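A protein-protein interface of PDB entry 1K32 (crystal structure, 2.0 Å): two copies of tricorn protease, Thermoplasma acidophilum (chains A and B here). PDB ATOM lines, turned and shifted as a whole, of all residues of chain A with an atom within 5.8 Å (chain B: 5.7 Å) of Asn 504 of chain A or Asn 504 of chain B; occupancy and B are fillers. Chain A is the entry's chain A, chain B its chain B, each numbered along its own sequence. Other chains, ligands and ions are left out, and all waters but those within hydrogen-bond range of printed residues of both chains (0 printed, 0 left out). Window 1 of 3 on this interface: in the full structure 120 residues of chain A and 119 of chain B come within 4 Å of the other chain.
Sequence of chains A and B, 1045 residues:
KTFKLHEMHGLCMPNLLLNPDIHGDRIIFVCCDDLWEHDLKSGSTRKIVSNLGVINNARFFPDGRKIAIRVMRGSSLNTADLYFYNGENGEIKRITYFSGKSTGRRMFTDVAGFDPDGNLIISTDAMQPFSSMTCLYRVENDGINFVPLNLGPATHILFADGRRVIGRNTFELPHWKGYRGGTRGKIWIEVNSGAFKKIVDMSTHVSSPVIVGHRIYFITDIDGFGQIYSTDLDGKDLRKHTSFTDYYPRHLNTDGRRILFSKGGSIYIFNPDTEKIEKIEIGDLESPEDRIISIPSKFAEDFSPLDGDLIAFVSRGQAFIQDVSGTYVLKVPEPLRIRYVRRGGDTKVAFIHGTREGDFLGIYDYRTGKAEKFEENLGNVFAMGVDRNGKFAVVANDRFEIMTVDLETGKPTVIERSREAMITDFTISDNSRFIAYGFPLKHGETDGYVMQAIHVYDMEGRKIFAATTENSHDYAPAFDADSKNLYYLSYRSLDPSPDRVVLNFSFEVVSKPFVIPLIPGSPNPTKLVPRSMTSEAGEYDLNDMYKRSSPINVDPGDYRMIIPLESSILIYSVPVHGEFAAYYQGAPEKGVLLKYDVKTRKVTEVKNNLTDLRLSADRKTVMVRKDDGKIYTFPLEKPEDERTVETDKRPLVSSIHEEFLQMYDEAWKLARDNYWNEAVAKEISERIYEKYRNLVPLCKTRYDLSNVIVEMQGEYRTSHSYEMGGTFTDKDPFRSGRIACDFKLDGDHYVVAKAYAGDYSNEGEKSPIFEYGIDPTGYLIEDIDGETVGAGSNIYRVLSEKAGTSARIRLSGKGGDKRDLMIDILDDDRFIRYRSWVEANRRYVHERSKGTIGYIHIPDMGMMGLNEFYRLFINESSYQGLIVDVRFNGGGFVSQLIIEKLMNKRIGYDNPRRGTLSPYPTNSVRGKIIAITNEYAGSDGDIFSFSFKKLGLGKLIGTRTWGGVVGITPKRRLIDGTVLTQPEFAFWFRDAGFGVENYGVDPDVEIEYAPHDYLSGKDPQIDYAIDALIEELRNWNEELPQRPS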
ATOM      1  N   TYR A 449       2.975  -9.029  12.298  1.00  0.00           N
ATOM      2  CA  TYR A 449       1.834  -8.191  12.625  1.00  0.00           C
ATOM      3  C   TYR A 449       2.020  -7.333  13.868  1.00  0.00           C
ATOM      4  O   TYR A 449       2.558  -7.775  14.887  1.00  0.00           O
ATOM      5  CB  TYR A 449       0.571  -9.047  12.782  1.00  0.00           C
ATOM      6  CG  TYR A 449       0.102  -9.690  11.497  1.00  0.00           C
ATOM      7  CD1 TYR A 449       0.643 -10.895  11.053  1.00  0.00           C
ATOM      8  CD2 TYR A 449      -0.869  -9.076  10.712  1.00  0.00           C
ATOM      9  CE1 TYR A 449       0.220 -11.475   9.851  1.00  0.00           C
ATOM     10  CE2 TYR A 449      -1.294  -9.639   9.515  1.00  0.00           C
ATOM     11  CZ  TYR A 449      -0.749 -10.834   9.088  1.00  0.00           C
ATOM     12  OH  TYR A 449      -1.166 -11.365   7.888  1.00  0.00           O
ATOM     13  N   SER A 497     -15.683 -14.550   5.647  1.00  0.00           N
ATOM     14  CA  SER A 497     -16.592 -14.279   4.535  1.00  0.00           C
ATOM     15  C   SER A 497     -15.987 -14.967   3.320  1.00  0.00           C
ATOM     16  O   SER A 497     -14.770 -15.007   3.182  1.00  0.00           O
ATOM     17  CB  SER A 497     -16.724 -12.780   4.298  1.00  0.00           C
ATOM     18  OG  SER A 497     -17.355 -12.171   5.401  1.00  0.00           O
ATOM     19  N   PRO A 498     -16.822 -15.533   2.426  1.00  0.00           N
ATOM     20  CA  PRO A 498     -16.247 -16.208   1.264  1.00  0.00           C
ATOM     21  C   PRO A 498     -15.980 -15.342   0.050  1.00  0.00           C
ATOM     22  O   PRO A 498     -16.733 -14.404  -0.243  1.00  0.00           O
ATOM     23  CB  PRO A 498     -17.271 -17.287   0.969  1.00  0.00           C
ATOM     24  CG  PRO A 498     -18.559 -16.543   1.204  1.00  0.00           C
ATOM     25  CD  PRO A 498     -18.279 -15.762   2.495  1.00  0.00           C
ATOM     26  N   ASP A 499     -14.884 -15.653  -0.640  1.00  0.00           N
ATOM     27  CA  ASP A 499     -14.517 -14.963  -1.871  1.00  0.00           C
ATOM     28  C   ASP A 499     -15.497 -15.561  -2.883  1.00  0.00           C
ATOM     29  O   ASP A 499     -15.781 -16.756  -2.817  1.00  0.00           O
ATOM     30  CB  ASP A 499     -13.077 -15.309  -2.277  1.00  0.00           C
ATOM     31  CG  ASP A 499     -12.614 -14.536  -3.511  1.00  0.00           C
ATOM     32  OD1 ASP A 499     -11.781 -13.619  -3.376  1.00  0.00           O
ATOM     33  OD2 ASP A 499     -13.082 -14.833  -4.619  1.00  0.00           O
ATOM     34  N   VAL A 502     -12.584 -16.837  -6.180  1.00  0.00           N
ATOM     35  CA  VAL A 502     -11.515 -17.776  -5.831  1.00  0.00           C
ATOM     36  C   VAL A 502     -11.800 -18.531  -4.531  1.00  0.00           C
ATOM     37  O   VAL A 502     -12.546 -18.053  -3.687  1.00  0.00           O
ATOM     38  CB  VAL A 502     -10.188 -16.988  -5.681  1.00  0.00           C
ATOM     39  CG1 VAL A 502      -9.038 -17.921  -5.358  1.00  0.00           C
ATOM     40  CG2 VAL A 502      -9.913 -16.197  -6.978  1.00  0.00           C
ATOM     41  N   LEU A 503     -11.234 -19.723  -4.376  1.00  0.00           N
ATOM     42  CA  LEU A 503     -11.416 -20.464  -3.123  1.00  0.00           C
ATOM     43  C   LEU A 503     -10.582 -19.658  -2.131  1.00  0.00           C
ATOM     44  O   LEU A 503      -9.347 -19.763  -2.103  1.00  0.00           O
ATOM     45  CB  LEU A 503     -10.844 -21.872  -3.205  1.00  0.00           C
ATOM     46  CG  LEU A 503     -10.915 -22.633  -1.873  1.00  0.00           C
ATOM     47  CD1 LEU A 503     -12.367 -22.786  -1.455  1.00  0.00           C
ATOM     48  CD2 LEU A 503     -10.252 -24.000  -2.017  1.00  0.00           C
ATOM     49  N   ASN A 504     -11.260 -18.872  -1.311  1.00  0.00           N
ATOM     50  CA  ASN A 504     -10.571 -18.003  -0.381  1.00  0.00           C
ATOM     51  C   ASN A 504     -11.608 -17.463   0.587  1.00  0.00           C
ATOM     52  O   ASN A 504     -12.803 -17.481   0.289  1.00  0.00           O
ATOM     53  CB  ASN A 504      -9.942 -16.863  -1.195  1.00  0.00           C
ATOM     54  CG  ASN A 504      -9.221 -15.827  -0.345  1.00  0.00           C
ATOM     55  OD1 ASN A 504      -9.233 -14.632  -0.674  1.00  0.00           O
ATOM     56  ND2 ASN A 504      -8.565 -16.267   0.721  1.00  0.00           N
ATOM     57  N   PHE A 505     -11.147 -17.019   1.750  1.00  0.00           N
ATOM     58  CA  PHE A 505     -12.011 -16.418   2.756  1.00  0.00           C
ATOM     59  C   PHE A 505     -11.251 -15.253   3.388  1.00  0.00           C
ATOM     60  O   PHE A 505     -10.015 -15.198   3.340  1.00  0.00           O
ATOM     61  CB  PHE A 505     -12.402 -17.436   3.834  1.00  0.00           C
ATOM     62  CG  PHE A 505     -13.333 -18.502   3.343  1.00  0.00           C
ATOM     63  CD1 PHE A 505     -12.854 -19.584   2.614  1.00  0.00           C
ATOM     64  CD2 PHE A 505     -14.699 -18.405   3.577  1.00  0.00           C
ATOM     65  CE1 PHE A 505     -13.717 -20.552   2.125  1.00  0.00           C
ATOM     66  CE2 PHE A 505     -15.576 -19.368   3.090  1.00  0.00           C
ATOM     67  CZ  PHE A 505     -15.086 -20.445   2.363  1.00  0.00           C
ATOM     68  N   SER A 506     -11.978 -14.305   3.961  1.00  0.00           N
ATOM     69  CA  SER A 506     -11.328 -13.176   4.600  1.00  0.00           C
ATOM     70  C   SER A 506     -12.236 -12.577   5.649  1.00  0.00           C
ATOM     71  O   SER A 506     -13.443 -12.744   5.592  1.00  0.00           O
ATOM     72  CB  SER A 506     -10.956 -12.109   3.573  1.00  0.00           C
ATOM     73  OG  SER A 506     -12.114 -11.539   3.012  1.00  0.00           O
ATOM     74  N   PHE A 507     -11.634 -11.870   6.598  1.00  0.00           N
ATOM     75  CA  PHE A 507     -12.356 -11.230   7.680  1.00  0.00           C
ATOM     76  C   PHE A 507     -12.784  -9.826   7.271  1.00  0.00           C
ATOM     77  O   PHE A 507     -12.000  -8.870   7.328  1.00  0.00           O
ATOM     78  CB  PHE A 507     -11.470 -11.206   8.928  1.00  0.00           C
ATOM     79  CG  PHE A 507     -11.013 -12.569   9.355  1.00  0.00           C
ATOM     80  CD1 PHE A 507      -9.674 -12.930   9.271  1.00  0.00           C
ATOM     81  CD2 PHE A 507     -11.929 -13.504   9.831  1.00  0.00           C
ATOM     82  CE1 PHE A 507      -9.250 -14.199   9.653  1.00  0.00           C
ATOM     83  CE2 PHE A 507     -11.515 -14.787  10.218  1.00  0.00           C
ATOM     84  CZ  PHE A 507     -10.173 -15.131  10.126  1.00  0.00           C
ATOM     85  N   LEU A 897       1.410 -12.307  -2.077  1.00  0.00           N
ATOM     86  CA  LEU A 897       0.155 -13.042  -2.138  1.00  0.00           C
ATOM     87  C   LEU A 897       0.131 -13.911  -3.401  1.00  0.00           C
ATOM     88  O   LEU A 897      -0.328 -15.064  -3.366  1.00  0.00           O
ATOM     89  CB  LEU A 897      -1.032 -12.075  -2.103  1.00  0.00           C
ATOM     90  CG  LEU A 897      -1.000 -11.100  -0.922  1.00  0.00           C
ATOM     91  CD1 LEU A 897      -2.205 -10.206  -0.965  1.00  0.00           C
ATOM     92  CD2 LEU A 897      -0.946 -11.885   0.399  1.00  0.00           C
ATOM     93  N   LYS A 901       0.332 -18.357  -3.924  1.00  0.00           N
ATOM     94  CA  LYS A 901      -0.502 -19.170  -4.801  1.00  0.00           C
ATOM     95  C   LYS A 901       0.360 -19.992  -5.744  1.00  0.00           C
ATOM     96  O   LYS A 901       0.155 -21.191  -5.911  1.00  0.00           O
ATOM     97  CB  LYS A 901      -1.402 -18.269  -5.645  1.00  0.00           C
ATOM     98  CG  LYS A 901      -2.859 -18.383  -5.326  1.00  0.00           C
ATOM     99  CD  LYS A 901      -3.146 -17.920  -3.932  1.00  0.00           C
ATOM    100  CE  LYS A 901      -4.645 -17.793  -3.725  1.00  0.00           C
ATOM    101  NZ  LYS A 901      -4.922 -17.172  -2.407  1.00  0.00           N
ATOM    102  N   ASN A 923      -6.130 -24.204  -5.689  1.00  0.00           N
ATOM    103  CA  ASN A 923      -5.309 -23.130  -6.246  1.00  0.00           C
ATOM    104  C   ASN A 923      -3.875 -23.558  -6.526  1.00  0.00           C
ATOM    105  O   ASN A 923      -2.928 -22.846  -6.188  1.00  0.00           O
ATOM    106  CB  ASN A 923      -5.284 -21.937  -5.298  1.00  0.00           C
ATOM    107  CG  ASN A 923      -6.595 -21.188  -5.264  1.00  0.00           C
ATOM    108  OD1 ASN A 923      -7.111 -20.860  -4.191  1.00  0.00           O
ATOM    109  ND2 ASN A 923      -7.136 -20.897  -6.434  1.00  0.00           N
ATOM    110  N   SER B 497     -11.316  -6.520  -1.963  1.00  0.00           N
ATOM    111  CA  SER B 497     -11.681  -5.933  -0.674  1.00  0.00           C
ATOM    112  C   SER B 497     -10.607  -6.412   0.318  1.00  0.00           C
ATOM    113  O   SER B 497     -10.200  -7.569   0.279  1.00  0.00           O
ATOM    114  CB  SER B 497     -13.055  -6.425  -0.222  1.00  0.00           C
ATOM    115  OG  SER B 497     -14.082  -5.926  -1.049  1.00  0.00           O
ATOM    116  N   PRO B 498     -10.139  -5.531   1.219  1.00  0.00           N
ATOM    117  CA  PRO B 498      -9.108  -5.981   2.156  1.00  0.00           C
ATOM    118  C   PRO B 498      -9.589  -6.692   3.411  1.00  0.00           C
ATOM    119  O   PRO B 498     -10.632  -6.358   3.979  1.00  0.00           O
ATOM    120  CB  PRO B 498      -8.376  -4.689   2.493  1.00  0.00           C
ATOM    121  CG  PRO B 498      -9.505  -3.707   2.568  1.00  0.00           C
ATOM    122  CD  PRO B 498     -10.378  -4.081   1.358  1.00  0.00           C
ATOM    123  N   ASP B 499      -8.812  -7.686   3.826  1.00  0.00           N
ATOM    124  CA  ASP B 499      -9.077  -8.429   5.048  1.00  0.00           C
ATOM    125  C   ASP B 499      -8.684  -7.431   6.140  1.00  0.00           C
ATOM    126  O   ASP B 499      -7.702  -6.688   5.982  1.00  0.00           O
ATOM    127  CB  ASP B 499      -8.174  -9.669   5.107  1.00  0.00           C
ATOM    128  CG  ASP B 499      -8.458 -10.558   6.320  1.00  0.00           C
ATOM    129  OD1 ASP B 499      -8.833 -11.732   6.122  1.00  0.00           O
ATOM    130  OD2 ASP B 499      -8.301 -10.102   7.469  1.00  0.00           O
ATOM    131  N   VAL B 502      -5.823 -10.085   8.685  1.00  0.00           N
ATOM    132  CA  VAL B 502      -4.690 -10.700   8.004  1.00  0.00           C
ATOM    133  C   VAL B 502      -4.358  -9.942   6.718  1.00  0.00           C
ATOM    134  O   VAL B 502      -5.200  -9.238   6.178  1.00  0.00           O
ATOM    135  CB  VAL B 502      -5.046 -12.168   7.658  1.00  0.00           C
ATOM    136  CG1 VAL B 502      -3.852 -12.882   7.043  1.00  0.00           C
ATOM    137  CG2 VAL B 502      -5.540 -12.894   8.925  1.00  0.00           C
ATOM    138  N   LEU B 503      -3.124 -10.068   6.244  1.00  0.00           N
ATOM    139  CA  LEU B 503      -2.737  -9.427   4.992  1.00  0.00           C
ATOM    140  C   LEU B 503      -3.365 -10.331   3.945  1.00  0.00           C
ATOM    141  O   LEU B 503      -2.822 -11.384   3.622  1.00  0.00           O
ATOM    142  CB  LEU B 503      -1.223  -9.440   4.806  1.00  0.00           C
ATOM    143  CG  LEU B 503      -0.774  -8.772   3.501  1.00  0.00           C
ATOM    144  CD1 LEU B 503      -1.147  -7.293   3.548  1.00  0.00           C
ATOM    145  CD2 LEU B 503       0.729  -8.944   3.294  1.00  0.00           C
ATOM    146  N   ASN B 504      -4.503  -9.916   3.411  1.00  0.00           N
ATOM    147  CA  ASN B 504      -5.212 -10.745   2.452  1.00  0.00           C
ATOM    148  C   ASN B 504      -6.279  -9.891   1.787  1.00  0.00           C
ATOM    149  O   ASN B 504      -6.696  -8.871   2.336  1.00  0.00           O
ATOM    150  CB  ASN B 504      -5.857 -11.909   3.221  1.00  0.00           C
ATOM    151  CG  ASN B 504      -6.672 -12.847   2.339  1.00  0.00           C
ATOM    152  OD1 ASN B 504      -7.653 -13.438   2.799  1.00  0.00           O
ATOM    153  ND2 ASN B 504      -6.266 -13.010   1.092  1.00  0.00           N
ATOM    154  N   PHE B 505      -6.704 -10.307   0.602  1.00  0.00           N
ATOM    155  CA  PHE B 505      -7.744  -9.614  -0.136  1.00  0.00           C
ATOM    156  C   PHE B 505      -8.674 -10.662  -0.747  1.00  0.00           C
ATOM    157  O   PHE B 505      -8.300 -11.826  -0.909  1.00  0.00           O
ATOM    158  CB  PHE B 505      -7.141  -8.741  -1.240  1.00  0.00           C
ATOM    159  CG  PHE B 505      -6.376  -7.565  -0.727  1.00  0.00           C
ATOM    160  CD1 PHE B 505      -5.052  -7.703  -0.308  1.00  0.00           C
ATOM    161  CD2 PHE B 505      -6.994  -6.325  -0.605  1.00  0.00           C
ATOM    162  CE1 PHE B 505      -4.357  -6.622   0.225  1.00  0.00           C
ATOM    163  CE2 PHE B 505      -6.301  -5.231  -0.068  1.00  0.00           C
ATOM    164  CZ  PHE B 505      -4.981  -5.383   0.347  1.00  0.00           C
ATOM    165  N   SER B 506      -9.899 -10.259  -1.060  1.00  0.00           N
ATOM    166  CA  SER B 506     -10.836 -11.189  -1.652  1.00  0.00           C
ATOM    167  C   SER B 506     -11.925 -10.452  -2.405  1.00  0.00           C
ATOM    168  O   SER B 506     -12.218  -9.294  -2.125  1.00  0.00           O
ATOM    169  CB  SER B 506     -11.474 -12.068  -0.582  1.00  0.00           C
ATOM    170  OG  SER B 506     -12.339 -11.296   0.219  1.00  0.00           O
ATOM    171  N   PHE B 507     -12.537 -11.158  -3.344  1.00  0.00           N
ATOM    172  CA  PHE B 507     -13.592 -10.604  -4.160  1.00  0.00           C
ATOM    173  C   PHE B 507     -14.952 -10.770  -3.486  1.00  0.00           C
ATOM    174  O   PHE B 507     -15.586 -11.828  -3.563  1.00  0.00           O
ATOM    175  CB  PHE B 507     -13.530 -11.273  -5.526  1.00  0.00           C
ATOM    176  CG  PHE B 507     -12.188 -11.129  -6.186  1.00  0.00           C
ATOM    177  CD1 PHE B 507     -11.395 -12.238  -6.437  1.00  0.00           C
ATOM    178  CD2 PHE B 507     -11.710  -9.871  -6.545  1.00  0.00           C
ATOM    179  CE1 PHE B 507     -10.150 -12.100  -7.038  1.00  0.00           C
ATOM    180  CE2 PHE B 507     -10.469  -9.727  -7.144  1.00  0.00           C
ATOM    181  CZ  PHE B 507      -9.691 -10.839  -7.390  1.00  0.00           C
ATOM    182  N   LEU B 897      -5.903 -24.104   2.581  1.00  0.00           N
ATOM    183  CA  LEU B 897      -5.658 -22.678   2.797  1.00  0.00           C
ATOM    184  C   LEU B 897      -4.648 -22.480   3.938  1.00  0.00           C
ATOM    185  O   LEU B 897      -3.756 -21.609   3.869  1.00  0.00           O
ATOM    186  CB  LEU B 897      -6.971 -21.959   3.109  1.00  0.00           C
ATOM    187  CG  LEU B 897      -8.075 -22.170   2.067  1.00  0.00           C
ATOM    188  CD1 LEU B 897      -9.284 -21.320   2.427  1.00  0.00           C
ATOM    189  CD2 LEU B 897      -7.550 -21.799   0.667  1.00  0.00           C
ATOM    190  N   LYS B 901      -0.444 -21.072   3.792  1.00  0.00           N
ATOM    191  CA  LYS B 901       0.161 -20.126   4.717  1.00  0.00           C
ATOM    192  C   LYS B 901       1.427 -20.719   5.340  1.00  0.00           C
ATOM    193  O   LYS B 901       2.478 -20.082   5.364  1.00  0.00           O
ATOM    194  CB  LYS B 901      -0.828 -19.809   5.842  1.00  0.00           C
ATOM    195  CG  LYS B 901      -1.332 -18.391   5.862  1.00  0.00           C
ATOM    196  CD  LYS B 901      -2.062 -18.060   4.589  1.00  0.00           C
ATOM    197  CE  LYS B 901      -2.626 -16.652   4.629  1.00  0.00           C
ATOM    198  NZ  LYS B 901      -3.328 -16.392   3.348  1.00  0.00           N
ATOM    199  N   ASN B 923       3.058 -13.134   5.996  1.00  0.00           N
ATOM    200  CA  ASN B 923       2.433 -14.350   6.520  1.00  0.00           C
ATOM    201  C   ASN B 923       3.378 -15.549   6.484  1.00  0.00           C
ATOM    202  O   ASN B 923       2.976 -16.642   6.097  1.00  0.00           O
ATOM    203  CB  ASN B 923       1.186 -14.729   5.715  1.00  0.00           C
ATOM    204  CG  ASN B 923      -0.004 -13.803   5.970  1.00  0.00           C
ATOM    205  OD1 ASN B 923      -0.666 -13.348   5.023  1.00  0.00           O
ATOM    206  ND2 ASN B 923      -0.296 -13.543   7.235  1.00  0.00           N
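The side-chain hydroxyl (OG) of Ser 506 of chain B lies within hydrogen-bond range of the side-chain hydroxyl (OG) of Ser 506 of chain A, at 2.8 Å.
The side-chain carboxylate of Asp 499 of chain A lies within hydrogen-bond range of the backbone NH of Phe 507 of chain B (2.6 Å).
The side-chain hydroxyl (OH) of Tyr 449 of chain A lies within hydrogen-bond range of the backbone NH (N) of Leu 503 of chain B, 2.9 Å away.
O of Phe 505 of chain A lies close to OD1 of Asn 504 of chain B.
The side-chain carboxylate (OD1) of Asp 499 of chain B is in hydrogen-bond range of the backbone NH (N) of Phe 507 of chain A, at 2.8 Å.
O of Phe 505 of chain B lies close to OD1 of Asn 504 of chain A (3.0 Å).
OH of Tyr 449 of chain A lies within hydrogen-bond range of ND2 of Asn 923 of chain B.
N of Asp 499 of chain A lies within hydrogen-bond range of O of Asn 504 of chain A (2.9 Å).
The side-chain amide oxygen (OD1) of Asn 923 of chain B lies close to the backbone carbonyl oxygen (O) of Leu 503 of chain B.
The backbone NH (N) of Val 502 of chain B is in hydrogen-bond range of the side-chain carboxylate (OD2) of Asp 499 of chain B, 2.8 Å away.
N of Asp 499 of chain B sits at hydrogen-bond distance from O of Asn 504 of chain B.
O of Leu 503 of chain A sits close to OD1 of Asn 923 of chain A (3.3 Å).
The backbone NH (N) of Ser 497 of chain B lies within hydrogen-bond range of the backbone carbonyl oxygen (O) of Ser 506 of chain B, at 2.9 Å.
Among the printed residues, merely in contact across the chains: Tyr 449 of chain A with Val 502 of chain B (3.2 Å), Asp 499 of chain A with Ser 506 of chain B (3.1 Å), Leu 503 of chain A with Leu 897 of chain B (3.9 Å), Asn 504 of chain A with Asn 504 of chain B (3.6 Å), Asn 504 of chain A with Ser 506 of chain B (3.4 Å), Phe 505 of chain A with Leu 897 of chain B (3.97 Å), Ser 506 of chain A with Asp 499 of chain B (3.3 Å), Ser 506 of chain A with Asn 504 of chain B (3.6 Å), Phe 507 of chain A with Val 502 of chain B (3.9996 Å), Leu 897 of chain A with Leu 503 of chain B (3.8 Å) and Leu 897 of chain A with Phe 505 of chain B (3.8 Å).
Asn 504 of chain A touches just these residues of chain B: Asn 504 (3.6 Å), Phe 505 (3.0 Å) and Ser 506 (3.4 Å).
Asn 504 of chain B touches three residues of chain A.
Printed residues of chain A within 4 Å of Val 502 of chain B: Tyr 449 (3.2 Å) and Phe 507 (3.9996 Å).
Of the printed residues of chain B, Phe 505 of chain A touches Asn 504 and Leu 897.
Printed residues of chain B within 4 Å of Leu 897 of chain A: Leu 503 and Phe 505.
Printed residues of chain A within 4 Å of Asn 923 of chain B: Tyr 449.
Lys 901 of chain B touches none of the printed residues of chain A.
The nearest residue of chain B that does not touch Asn 504 of chain A is Leu 897 of chain B (4.5 Å).
The nearest printed residue of chain A that does not touch Leu 897 of chain B is Asn 504 of chain A (4.5 Å).
Of the 13 printed residues of chain A, 8 touch a printed residue of chain B.
Printed residues of chain A that touch a printed residue of chain B: Tyr 449, Asp 499, Leu 503, Asn 504, Phe 505, Ser 506, Phe 507 and Leu 897.
Of the 12 printed residues of chain B, 9 touch a printed residue of chain A.
Hydrophobic or aromatic side chains of chain B within 4 Å of the printed part of chain A: Val 502, Leu 503, Phe 505, Phe 507 and Leu 897.
Among the printed residues, no Asp or Glu carboxylate lies within 4 Å of a Lys or Arg side-chain nitrogen of the other chain.
Asp 499 of chain A touches Ser 506 of chain B, and with the chains exchanged Ser 506 of chain A touches Asp 499 of chain B.
Leu 503 of chain A touches Leu 897 of chain B, and with the chains exchanged Leu 897 of chain A touches Leu 503 of chain B.
Ser 506 of chain B touches its own counterpart, Ser 506 of chain A.
Phe 507 of chain A touches Val 502 of chain B, but with the chains exchanged Val 502 of chain A does not touch Phe 507 of chain B (4.1 Å).
Of the 18 pairs that touch across the chains among the printed residues, 14 have their exchanged pair printed and touching as well.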
